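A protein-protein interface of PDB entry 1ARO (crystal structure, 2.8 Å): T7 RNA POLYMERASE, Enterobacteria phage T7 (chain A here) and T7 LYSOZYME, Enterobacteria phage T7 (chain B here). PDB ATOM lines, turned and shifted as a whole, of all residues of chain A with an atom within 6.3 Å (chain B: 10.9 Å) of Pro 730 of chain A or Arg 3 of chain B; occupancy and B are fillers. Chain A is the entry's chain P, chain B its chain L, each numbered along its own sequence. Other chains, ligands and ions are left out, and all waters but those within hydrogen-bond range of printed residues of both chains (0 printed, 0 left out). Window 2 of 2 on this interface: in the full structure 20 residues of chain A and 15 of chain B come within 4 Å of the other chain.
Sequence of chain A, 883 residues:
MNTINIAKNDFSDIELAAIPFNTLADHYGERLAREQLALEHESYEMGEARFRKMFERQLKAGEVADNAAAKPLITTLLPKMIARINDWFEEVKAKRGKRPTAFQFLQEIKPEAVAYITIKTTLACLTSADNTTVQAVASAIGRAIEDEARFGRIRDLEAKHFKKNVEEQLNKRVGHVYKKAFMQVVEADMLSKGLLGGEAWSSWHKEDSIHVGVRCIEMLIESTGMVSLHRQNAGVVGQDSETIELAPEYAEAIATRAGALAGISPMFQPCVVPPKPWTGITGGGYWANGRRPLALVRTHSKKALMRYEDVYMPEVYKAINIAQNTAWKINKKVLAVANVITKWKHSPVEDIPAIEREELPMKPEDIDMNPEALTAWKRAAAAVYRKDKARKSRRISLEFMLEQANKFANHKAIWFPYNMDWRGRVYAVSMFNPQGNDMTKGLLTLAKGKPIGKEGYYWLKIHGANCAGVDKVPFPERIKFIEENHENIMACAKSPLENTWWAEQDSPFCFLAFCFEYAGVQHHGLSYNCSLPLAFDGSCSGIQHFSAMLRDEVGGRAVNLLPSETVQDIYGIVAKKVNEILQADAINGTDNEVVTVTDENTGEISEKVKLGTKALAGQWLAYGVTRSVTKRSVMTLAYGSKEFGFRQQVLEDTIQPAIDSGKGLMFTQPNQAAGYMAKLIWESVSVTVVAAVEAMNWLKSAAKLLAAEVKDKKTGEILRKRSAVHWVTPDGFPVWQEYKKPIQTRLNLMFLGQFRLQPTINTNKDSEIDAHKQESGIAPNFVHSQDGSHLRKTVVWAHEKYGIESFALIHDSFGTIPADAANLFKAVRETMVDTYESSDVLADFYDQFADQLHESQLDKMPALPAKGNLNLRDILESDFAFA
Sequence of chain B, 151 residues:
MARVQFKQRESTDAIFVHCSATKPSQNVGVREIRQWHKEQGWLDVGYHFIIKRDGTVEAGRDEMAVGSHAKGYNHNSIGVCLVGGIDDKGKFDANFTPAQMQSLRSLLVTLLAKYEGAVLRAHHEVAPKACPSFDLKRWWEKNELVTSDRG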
ATOM      1  N   VAL A 728      14.452  28.529 -30.180  1.00  0.00           N
ATOM      2  CA  VAL A 728      14.163  27.079 -30.129  1.00  0.00           C
ATOM      3  C   VAL A 728      13.262  26.529 -29.025  1.00  0.00           C
ATOM      4  O   VAL A 728      13.520  26.716 -27.837  1.00  0.00           O
ATOM      5  CB  VAL A 728      15.431  26.206 -30.037  1.00  0.00           C
ATOM      6  CG1 VAL A 728      15.166  24.865 -30.757  1.00  0.00           C
ATOM      7  CG2 VAL A 728      16.620  26.918 -30.631  1.00  0.00           C
ATOM      8  N   THR A 729      12.219  25.814 -29.432  1.00  0.00           N
ATOM      9  CA  THR A 729      11.311  25.171 -28.493  1.00  0.00           C
ATOM     10  C   THR A 729      12.027  24.030 -27.759  1.00  0.00           C
ATOM     11  O   THR A 729      13.013  23.469 -28.260  1.00  0.00           O
ATOM     12  CB  THR A 729      10.166  24.490 -29.206  1.00  0.00           C
ATOM     13  OG1 THR A 729      10.690  23.376 -29.958  1.00  0.00           O
ATOM     14  CG2 THR A 729       9.427  25.484 -30.105  1.00  0.00           C
ATOM     15  N   PRO A 730      11.515  23.643 -26.573  1.00  0.00           N
ATOM     16  CA  PRO A 730      12.099  22.557 -25.771  1.00  0.00           C
ATOM     17  C   PRO A 730      12.324  21.184 -26.466  1.00  0.00           C
ATOM     18  O   PRO A 730      13.304  20.502 -26.174  1.00  0.00           O
ATOM     19  CB  PRO A 730      11.160  22.495 -24.577  1.00  0.00           C
ATOM     20  CG  PRO A 730      10.770  23.976 -24.436  1.00  0.00           C
ATOM     21  CD  PRO A 730      10.369  24.224 -25.860  1.00  0.00           C
ATOM     22  N   ASP A 731      11.464  20.772 -27.393  1.00  0.00           N
ATOM     23  CA  ASP A 731      11.729  19.505 -28.065  1.00  0.00           C
ATOM     24  C   ASP A 731      12.833  19.640 -29.117  1.00  0.00           C
ATOM     25  O   ASP A 731      13.137  18.689 -29.838  1.00  0.00           O
ATOM     26  CB  ASP A 731      10.453  18.924 -28.701  1.00  0.00           C
ATOM     27  CG  ASP A 731       9.872  19.799 -29.790  1.00  0.00           C
ATOM     28  OD1 ASP A 731       9.438  20.932 -29.492  1.00  0.00           O
ATOM     29  OD2 ASP A 731       9.843  19.347 -30.958  1.00  0.00           O
ATOM     30  N   GLY A 732      13.427  20.826 -29.219  1.00  0.00           N
ATOM     31  CA  GLY A 732      14.508  21.014 -30.170  1.00  0.00           C
ATOM     32  C   GLY A 732      14.226  21.690 -31.508  1.00  0.00           C
ATOM     33  O   GLY A 732      15.160  22.047 -32.202  1.00  0.00           O
ATOM     34  N   PHE A 733      12.958  21.873 -31.869  1.00  0.00           N
ATOM     35  CA  PHE A 733      12.600  22.510 -33.127  1.00  0.00           C
ATOM     36  C   PHE A 733      12.950  24.007 -33.164  1.00  0.00           C
ATOM     37  O   PHE A 733      12.487  24.765 -32.312  1.00  0.00           O
ATOM     38  CB  PHE A 733      11.112  22.353 -33.340  1.00  0.00           C
ATOM     39  CG  PHE A 733      10.626  22.914 -34.643  1.00  0.00           C
ATOM     40  CD1 PHE A 733      10.831  22.231 -35.832  1.00  0.00           C
ATOM     41  CD2 PHE A 733       9.964  24.121 -34.685  1.00  0.00           C
ATOM     42  CE1 PHE A 733      10.378  22.744 -37.044  1.00  0.00           C
ATOM     43  CE2 PHE A 733       9.512  24.638 -35.898  1.00  0.00           C
ATOM     44  CZ  PHE A 733       9.722  23.940 -37.076  1.00  0.00           C
ATOM     45  N   SER A 789       5.017  22.880 -29.660  1.00  0.00           N
ATOM     46  CA  SER A 789       5.918  22.110 -28.857  1.00  0.00           C
ATOM     47  C   SER A 789       5.300  21.456 -27.635  1.00  0.00           C
ATOM     48  O   SER A 789       5.960  20.649 -27.007  1.00  0.00           O
ATOM     49  CB  SER A 789       7.086  22.981 -28.441  1.00  0.00           C
ATOM     50  OG  SER A 789       8.139  22.208 -27.915  1.00  0.00           O
ATOM     51  N   LYS A 793       5.202  17.110 -27.598  1.00  0.00           N
ATOM     52  CA  LYS A 793       5.702  16.491 -26.381  1.00  0.00           C
ATOM     53  C   LYS A 793       4.696  15.558 -25.710  1.00  0.00           C
ATOM     54  O   LYS A 793       5.045  14.461 -25.241  1.00  0.00           O
ATOM     55  CB  LYS A 793       6.187  17.564 -25.385  1.00  0.00           C
ATOM     56  CG  LYS A 793       7.503  18.214 -25.820  1.00  0.00           C
ATOM     57  CD  LYS A 793       8.108  19.177 -24.796  1.00  0.00           C
ATOM     58  CE  LYS A 793       8.580  18.481 -23.514  1.00  0.00           C
ATOM     59  NZ  LYS A 793       7.452  17.879 -22.761  1.00  0.00           N
ATOM     60  N   THR A 835       7.846  19.916 -17.872  1.00  0.00           N
ATOM     61  CA  THR A 835       8.511  21.000 -18.580  1.00  0.00           C
ATOM     62  C   THR A 835       9.050  22.094 -17.681  1.00  0.00           C
ATOM     63  O   THR A 835      10.245  22.371 -17.653  1.00  0.00           O
ATOM     64  CB  THR A 835       7.569  21.659 -19.584  1.00  0.00           C
ATOM     65  OG1 THR A 835       6.997  20.662 -20.440  1.00  0.00           O
ATOM     66  CG2 THR A 835       8.338  22.649 -20.424  1.00  0.00           C
ATOM     67  N   VAL A 841      12.310  27.648 -18.319  1.00  0.00           N
ATOM     68  CA  VAL A 841      12.301  27.996 -19.723  1.00  0.00           C
ATOM     69  C   VAL A 841      12.368  29.480 -20.006  1.00  0.00           C
ATOM     70  O   VAL A 841      13.037  29.881 -20.953  1.00  0.00           O
ATOM     71  CB  VAL A 841      11.101  27.376 -20.471  1.00  0.00           C
ATOM     72  CG1 VAL A 841      11.180  25.863 -20.377  1.00  0.00           C
ATOM     73  CG2 VAL A 841       9.813  27.883 -19.911  1.00  0.00           C
ATOM     74  N   ASP A 844      15.837  30.501 -19.803  1.00  0.00           N
ATOM     75  CA  ASP A 844      16.538  30.006 -20.984  1.00  0.00           C
ATOM     76  C   ASP A 844      16.261  30.914 -22.177  1.00  0.00           C
ATOM     77  O   ASP A 844      17.191  31.307 -22.886  1.00  0.00           O
ATOM     78  CB  ASP A 844      16.088  28.591 -21.352  1.00  0.00           C
ATOM     79  CG  ASP A 844      16.967  27.964 -22.423  1.00  0.00           C
ATOM     80  OD1 ASP A 844      17.405  28.691 -23.337  1.00  0.00           O
ATOM     81  OD2 ASP A 844      17.202  26.741 -22.367  1.00  0.00           O
ATOM     82  N   PHE A 845      14.989  31.238 -22.413  1.00  0.00           N
ATOM     83  CA  PHE A 845      14.664  32.101 -23.527  1.00  0.00           C
ATOM     84  C   PHE A 845      15.349  33.428 -23.361  1.00  0.00           C
ATOM     85  O   PHE A 845      15.714  34.082 -24.352  1.00  0.00           O
ATOM     86  CB  PHE A 845      13.169  32.296 -23.669  1.00  0.00           C
ATOM     87  CG  PHE A 845      12.488  31.159 -24.371  1.00  0.00           C
ATOM     88  CD1 PHE A 845      12.585  31.022 -25.756  1.00  0.00           C
ATOM     89  CD2 PHE A 845      11.764  30.220 -23.660  1.00  0.00           C
ATOM     90  CE1 PHE A 845      11.967  29.974 -26.406  1.00  0.00           C
ATOM     91  CE2 PHE A 845      11.141  29.169 -24.297  1.00  0.00           C
ATOM     92  CZ  PHE A 845      11.241  29.044 -25.674  1.00  0.00           C
ATOM     93  N   GLN A 848      18.702  32.922 -24.599  1.00  0.00           N
ATOM     94  CA  GLN A 848      18.526  32.692 -26.022  1.00  0.00           C
ATOM     95  C   GLN A 848      18.424  33.972 -26.840  1.00  0.00           C
ATOM     96  O   GLN A 848      18.997  34.082 -27.932  1.00  0.00           O
ATOM     97  CB  GLN A 848      17.297  31.815 -26.268  1.00  0.00           C
ATOM     98  CG  GLN A 848      17.657  30.387 -26.578  1.00  0.00           C
ATOM     99  CD  GLN A 848      16.483  29.608 -27.102  1.00  0.00           C
ATOM    100  OE1 GLN A 848      15.587  29.247 -26.358  1.00  0.00           O
ATOM    101  NE2 GLN A 848      16.469  29.363 -28.410  1.00  0.00           N
ATOM    102  N   ARG B   3      21.390  26.843 -28.008  1.00  0.00           N
ATOM    103  CA  ARG B   3      20.342  25.883 -27.556  1.00  0.00           C
ATOM    104  C   ARG B   3      19.961  24.921 -28.683  1.00  0.00           C
ATOM    105  O   ARG B   3      19.510  23.796 -28.442  1.00  0.00           O
ATOM    106  CB  ARG B   3      19.107  26.638 -27.102  1.00  0.00           C
ATOM    107  CG  ARG B   3      18.100  25.750 -26.487  1.00  0.00           C
ATOM    108  CD  ARG B   3      18.523  25.330 -25.104  1.00  0.00           C
ATOM    109  NE  ARG B   3      17.702  24.194 -24.670  1.00  0.00           N
ATOM    110  CZ  ARG B   3      16.403  24.056 -24.857  1.00  0.00           C
ATOM    111  NH1 ARG B   3      15.681  24.985 -25.486  1.00  0.00           N
ATOM    112  NH2 ARG B   3      15.803  22.946 -24.431  1.00  0.00           N
ATOM    113  N   VAL B   4      20.109  25.385 -29.917  1.00  0.00           N
ATOM    114  CA  VAL B   4      19.839  24.560 -31.083  1.00  0.00           C
ATOM    115  C   VAL B   4      21.009  23.590 -31.165  1.00  0.00           C
ATOM    116  O   VAL B   4      22.155  23.981 -30.974  1.00  0.00           O
ATOM    117  CB  VAL B   4      19.800  25.417 -32.334  1.00  0.00           C
ATOM    118  CG1 VAL B   4      20.930  26.414 -32.289  1.00  0.00           C
ATOM    119  CG2 VAL B   4      19.941  24.564 -33.561  1.00  0.00           C
ATOM    120  N   GLN B   5      20.716  22.324 -31.441  1.00  0.00           N
ATOM    121  CA  GLN B   5      21.732  21.279 -31.520  1.00  0.00           C
ATOM    122  C   GLN B   5      21.933  20.810 -32.957  1.00  0.00           C
ATOM    123  O   GLN B   5      20.957  20.696 -33.706  1.00  0.00           O
ATOM    124  CB  GLN B   5      21.284  20.079 -30.679  1.00  0.00           C
ATOM    125  CG  GLN B   5      22.022  19.852 -29.372  1.00  0.00           C
ATOM    126  CD  GLN B   5      21.617  18.516 -28.700  1.00  0.00           C
ATOM    127  OE1 GLN B   5      20.562  18.419 -28.064  1.00  0.00           O
ATOM    128  NE2 GLN B   5      22.453  17.479 -28.871  1.00  0.00           N
ATOM    129  N   PHE B   6      23.180  20.538 -33.353  1.00  0.00           N
ATOM    130  CA  PHE B   6      23.435  20.011 -34.708  1.00  0.00           C
ATOM    131  C   PHE B   6      23.937  18.549 -34.637  1.00  0.00           C
ATOM    132  O   PHE B   6      24.495  18.130 -33.613  1.00  0.00           O
ATOM    133  CB  PHE B   6      24.503  20.826 -35.451  1.00  0.00           C
ATOM    134  CG  PHE B   6      24.186  22.282 -35.595  1.00  0.00           C
ATOM    135  CD1 PHE B   6      23.465  22.746 -36.688  1.00  0.00           C
ATOM    136  CD2 PHE B   6      24.594  23.191 -34.631  1.00  0.00           C
ATOM    137  CE1 PHE B   6      23.152  24.099 -36.815  1.00  0.00           C
ATOM    138  CE2 PHE B   6      24.285  24.552 -34.749  1.00  0.00           C
ATOM    139  CZ  PHE B   6      23.562  25.003 -35.844  1.00  0.00           C
ATOM    140  N   LYS B   7      23.756  17.786 -35.717  1.00  0.00           N
ATOM    141  CA  LYS B   7      24.224  16.389 -35.787  1.00  0.00           C
ATOM    142  C   LYS B   7      25.696  16.229 -35.428  1.00  0.00           C
ATOM    143  O   LYS B   7      26.420  17.204 -35.302  1.00  0.00           O
ATOM    144  CB  LYS B   7      24.006  15.813 -37.193  1.00  0.00           C
ATOM    145  CG  LYS B   7      22.544  15.641 -37.560  1.00  0.00           C
ATOM    146  CD  LYS B   7      22.322  15.267 -39.024  1.00  0.00           C
ATOM    147  CE  LYS B   7      20.814  15.152 -39.332  1.00  0.00           C
ATOM    148  NZ  LYS B   7      20.514  14.854 -40.761  1.00  0.00           N
ATOM    149  N   ARG B  34      28.835  35.794 -34.866  1.00  0.00           N
ATOM    150  CA  ARG B  34      27.580  35.079 -35.023  1.00  0.00           C
ATOM    151  C   ARG B  34      26.568  35.978 -35.729  1.00  0.00           C
ATOM    152  O   ARG B  34      25.756  35.512 -36.539  1.00  0.00           O
ATOM    153  CB  ARG B  34      27.043  34.642 -33.662  1.00  0.00           C
ATOM    154  CG  ARG B  34      25.709  33.971 -33.765  1.00  0.00           C
ATOM    155  CD  ARG B  34      25.162  33.630 -32.407  1.00  0.00           C
ATOM    156  NE  ARG B  34      25.944  32.610 -31.719  1.00  0.00           N
ATOM    157  CZ  ARG B  34      26.568  32.813 -30.572  1.00  0.00           C
ATOM    158  NH1 ARG B  34      26.503  34.014 -29.984  1.00  0.00           N
ATOM    159  NH2 ARG B  34      27.236  31.805 -30.015  1.00  0.00           N
ATOM    160  N   LEU B  43      21.470  29.362 -38.286  1.00  0.00           N
ATOM    161  CA  LEU B  43      20.980  29.149 -36.922  1.00  0.00           C
ATOM    162  C   LEU B  43      22.043  29.336 -35.839  1.00  0.00           C
ATOM    163  O   LEU B  43      21.705  29.498 -34.668  1.00  0.00           O
ATOM    164  CB  LEU B  43      20.369  27.745 -36.804  1.00  0.00           C
ATOM    165  CG  LEU B  43      19.080  27.462 -37.602  1.00  0.00           C
ATOM    166  CD1 LEU B  43      18.702  25.962 -37.596  1.00  0.00           C
ATOM    167  CD2 LEU B  43      17.964  28.308 -36.996  1.00  0.00           C
ATOM    168  N   ASP B  44      23.321  29.305 -36.231  1.00  0.00           N
ATOM    169  CA  ASP B  44      24.433  29.495 -35.284  1.00  0.00           C
ATOM    170  C   ASP B  44      25.814  29.700 -35.936  1.00  0.00           C
ATOM    171  O   ASP B  44      26.033  29.349 -37.086  1.00  0.00           O
ATOM    172  CB  ASP B  44      24.535  28.300 -34.353  1.00  0.00           C
ATOM    173  CG  ASP B  44      25.194  28.648 -33.045  1.00  0.00           C
ATOM    174  OD1 ASP B  44      25.899  29.683 -32.979  1.00  0.00           O
ATOM    175  OD2 ASP B  44      25.008  27.871 -32.083  1.00  0.00           O
ATOM    176  N   VAL B  45      26.769  30.234 -35.192  1.00  0.00           N
ATOM    177  CA  VAL B  45      28.095  30.442 -35.760  1.00  0.00           C
ATOM    178  C   VAL B  45      28.611  29.156 -36.376  1.00  0.00           C
ATOM    179  O   VAL B  45      28.342  28.085 -35.860  1.00  0.00           O
ATOM    180  CB  VAL B  45      29.106  30.944 -34.712  1.00  0.00           C
ATOM    181  CG1 VAL B  45      29.293  29.932 -33.606  1.00  0.00           C
ATOM    182  CG2 VAL B  45      30.406  31.239 -35.398  1.00  0.00           C
ATOM    183  N   ALA B  59      34.381  29.455 -27.046  1.00  0.00           N
ATOM    184  CA  ALA B  59      33.828  28.253 -27.648  1.00  0.00           C
ATOM    185  C   ALA B  59      32.598  28.551 -28.500  1.00  0.00           C
ATOM    186  O   ALA B  59      31.666  29.214 -28.040  1.00  0.00           O
ATOM    187  CB  ALA B  59      33.456  27.295 -26.568  1.00  0.00           C
ATOM    188  N   GLY B  60      32.589  28.038 -29.732  1.00  0.00           N
ATOM    189  CA  GLY B  60      31.457  28.220 -30.643  1.00  0.00           C
ATOM    190  C   GLY B  60      30.534  27.004 -30.641  1.00  0.00           C
ATOM    191  O   GLY B  60      30.049  26.590 -29.581  1.00  0.00           O
ATOM    192  N   ARG B  61      30.274  26.413 -31.800  1.00  0.00           N
ATOM    193  CA  ARG B  61      29.427  25.223 -31.840  1.00  0.00           C
ATOM    194  C   ARG B  61      30.085  24.120 -31.049  1.00  0.00           C
ATOM    195  O   ARG B  61      31.291  24.142 -30.819  1.00  0.00           O
ATOM    196  CB  ARG B  61      29.246  24.678 -33.247  1.00  0.00           C
ATOM    197  CG  ARG B  61      28.460  25.533 -34.172  1.00  0.00           C
ATOM    198  CD  ARG B  61      28.227  24.736 -35.389  1.00  0.00           C
ATOM    199  NE  ARG B  61      27.471  25.481 -36.368  1.00  0.00           N
ATOM    200  CZ  ARG B  61      26.998  24.932 -37.473  1.00  0.00           C
ATOM    201  NH1 ARG B  61      27.222  23.646 -37.696  1.00  0.00           N
ATOM    202  NH2 ARG B  61      26.331  25.661 -38.357  1.00  0.00           N
ATOM    203  N   ASP B  62      29.291  23.133 -30.661  1.00  0.00           N
ATOM    204  CA  ASP B  62      29.808  22.027 -29.885  1.00  0.00           C
ATOM    205  C   ASP B  62      30.988  21.385 -30.601  1.00  0.00           C
ATOM    206  O   ASP B  62      30.886  21.106 -31.786  1.00  0.00           O
ATOM    207  CB  ASP B  62      28.722  20.970 -29.704  1.00  0.00           C
ATOM    208  CG  ASP B  62      28.992  20.031 -28.526  1.00  0.00           C
ATOM    209  OD1 ASP B  62      30.145  19.619 -28.304  1.00  0.00           O
ATOM    210  OD2 ASP B  62      28.029  19.683 -27.823  1.00  0.00           O
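Of the 13 printed residues of chain A, 4 touch a printed residue of chain B. Printed residues of chain A that touch a printed residue of chain B: Val 728, Pro 730, Asp 844 and Gln 848. Hydrophobic or aromatic side chains of chain A within 4 Å of the printed part of chain B: Val 728. Hydrophobic or aromatic side chains of chain B that line the printed part of chain A: Val 4. Among the printed residues, Asp or Glu carboxylates within 4 Å of a Lys or Arg side-chain nitrogen of the other chain: Asp 844 of chain A with Arg 3 of chain B (3.5 Å).
The side-chain amide nitrogen of Gln 848 of chain A sits close to the backbone NH of Val 728 of chain A.
Arg 3 of chain B touches Val 728 of chain A. Val 4 of chain B touches Val 728 of chain A. Arg 3 of chain B touches Pro 730 of chain A. CD of Gln 848 of chain A touches CB of Arg 3 of chain B (3.96 Å).
The side-chain carboxylate (OD2) of Asp 844 of chain A lies within salt-bridge range of the guanidinium group (NE) of Arg 3 of chain B, 3.5 Å away.
Printed residues of chain B within 4 Å of Pro 730 of chain A: Arg 3. Of chain A, only Val 728 (3.6 Å), Pro 730 (3.9 Å), Asp 844 (3.4 Å) and Gln 848 (3.96 Å) come within 4 Å of Arg 3 of chain B. No residue of chain B comes within 4 Å of Thr 729 of chain A. No residue of chain B comes within 4 Å of Ser 789 of chain A. Of the printed residues of chain B, Asp 844 of chain A touches Arg 3. Of the printed residues of chain B, Gln 848 of chain A touches Arg 3. Of the printed residues of chain A, Val 4 of chain B touches Val 728 (3.9 Å). Phe 845 of chain A touches none of the printed residues of chain B. The nearest printed residue of chain B that does not touch Gln 848 of chain A is Val 4 of chain B (5.6 Å).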
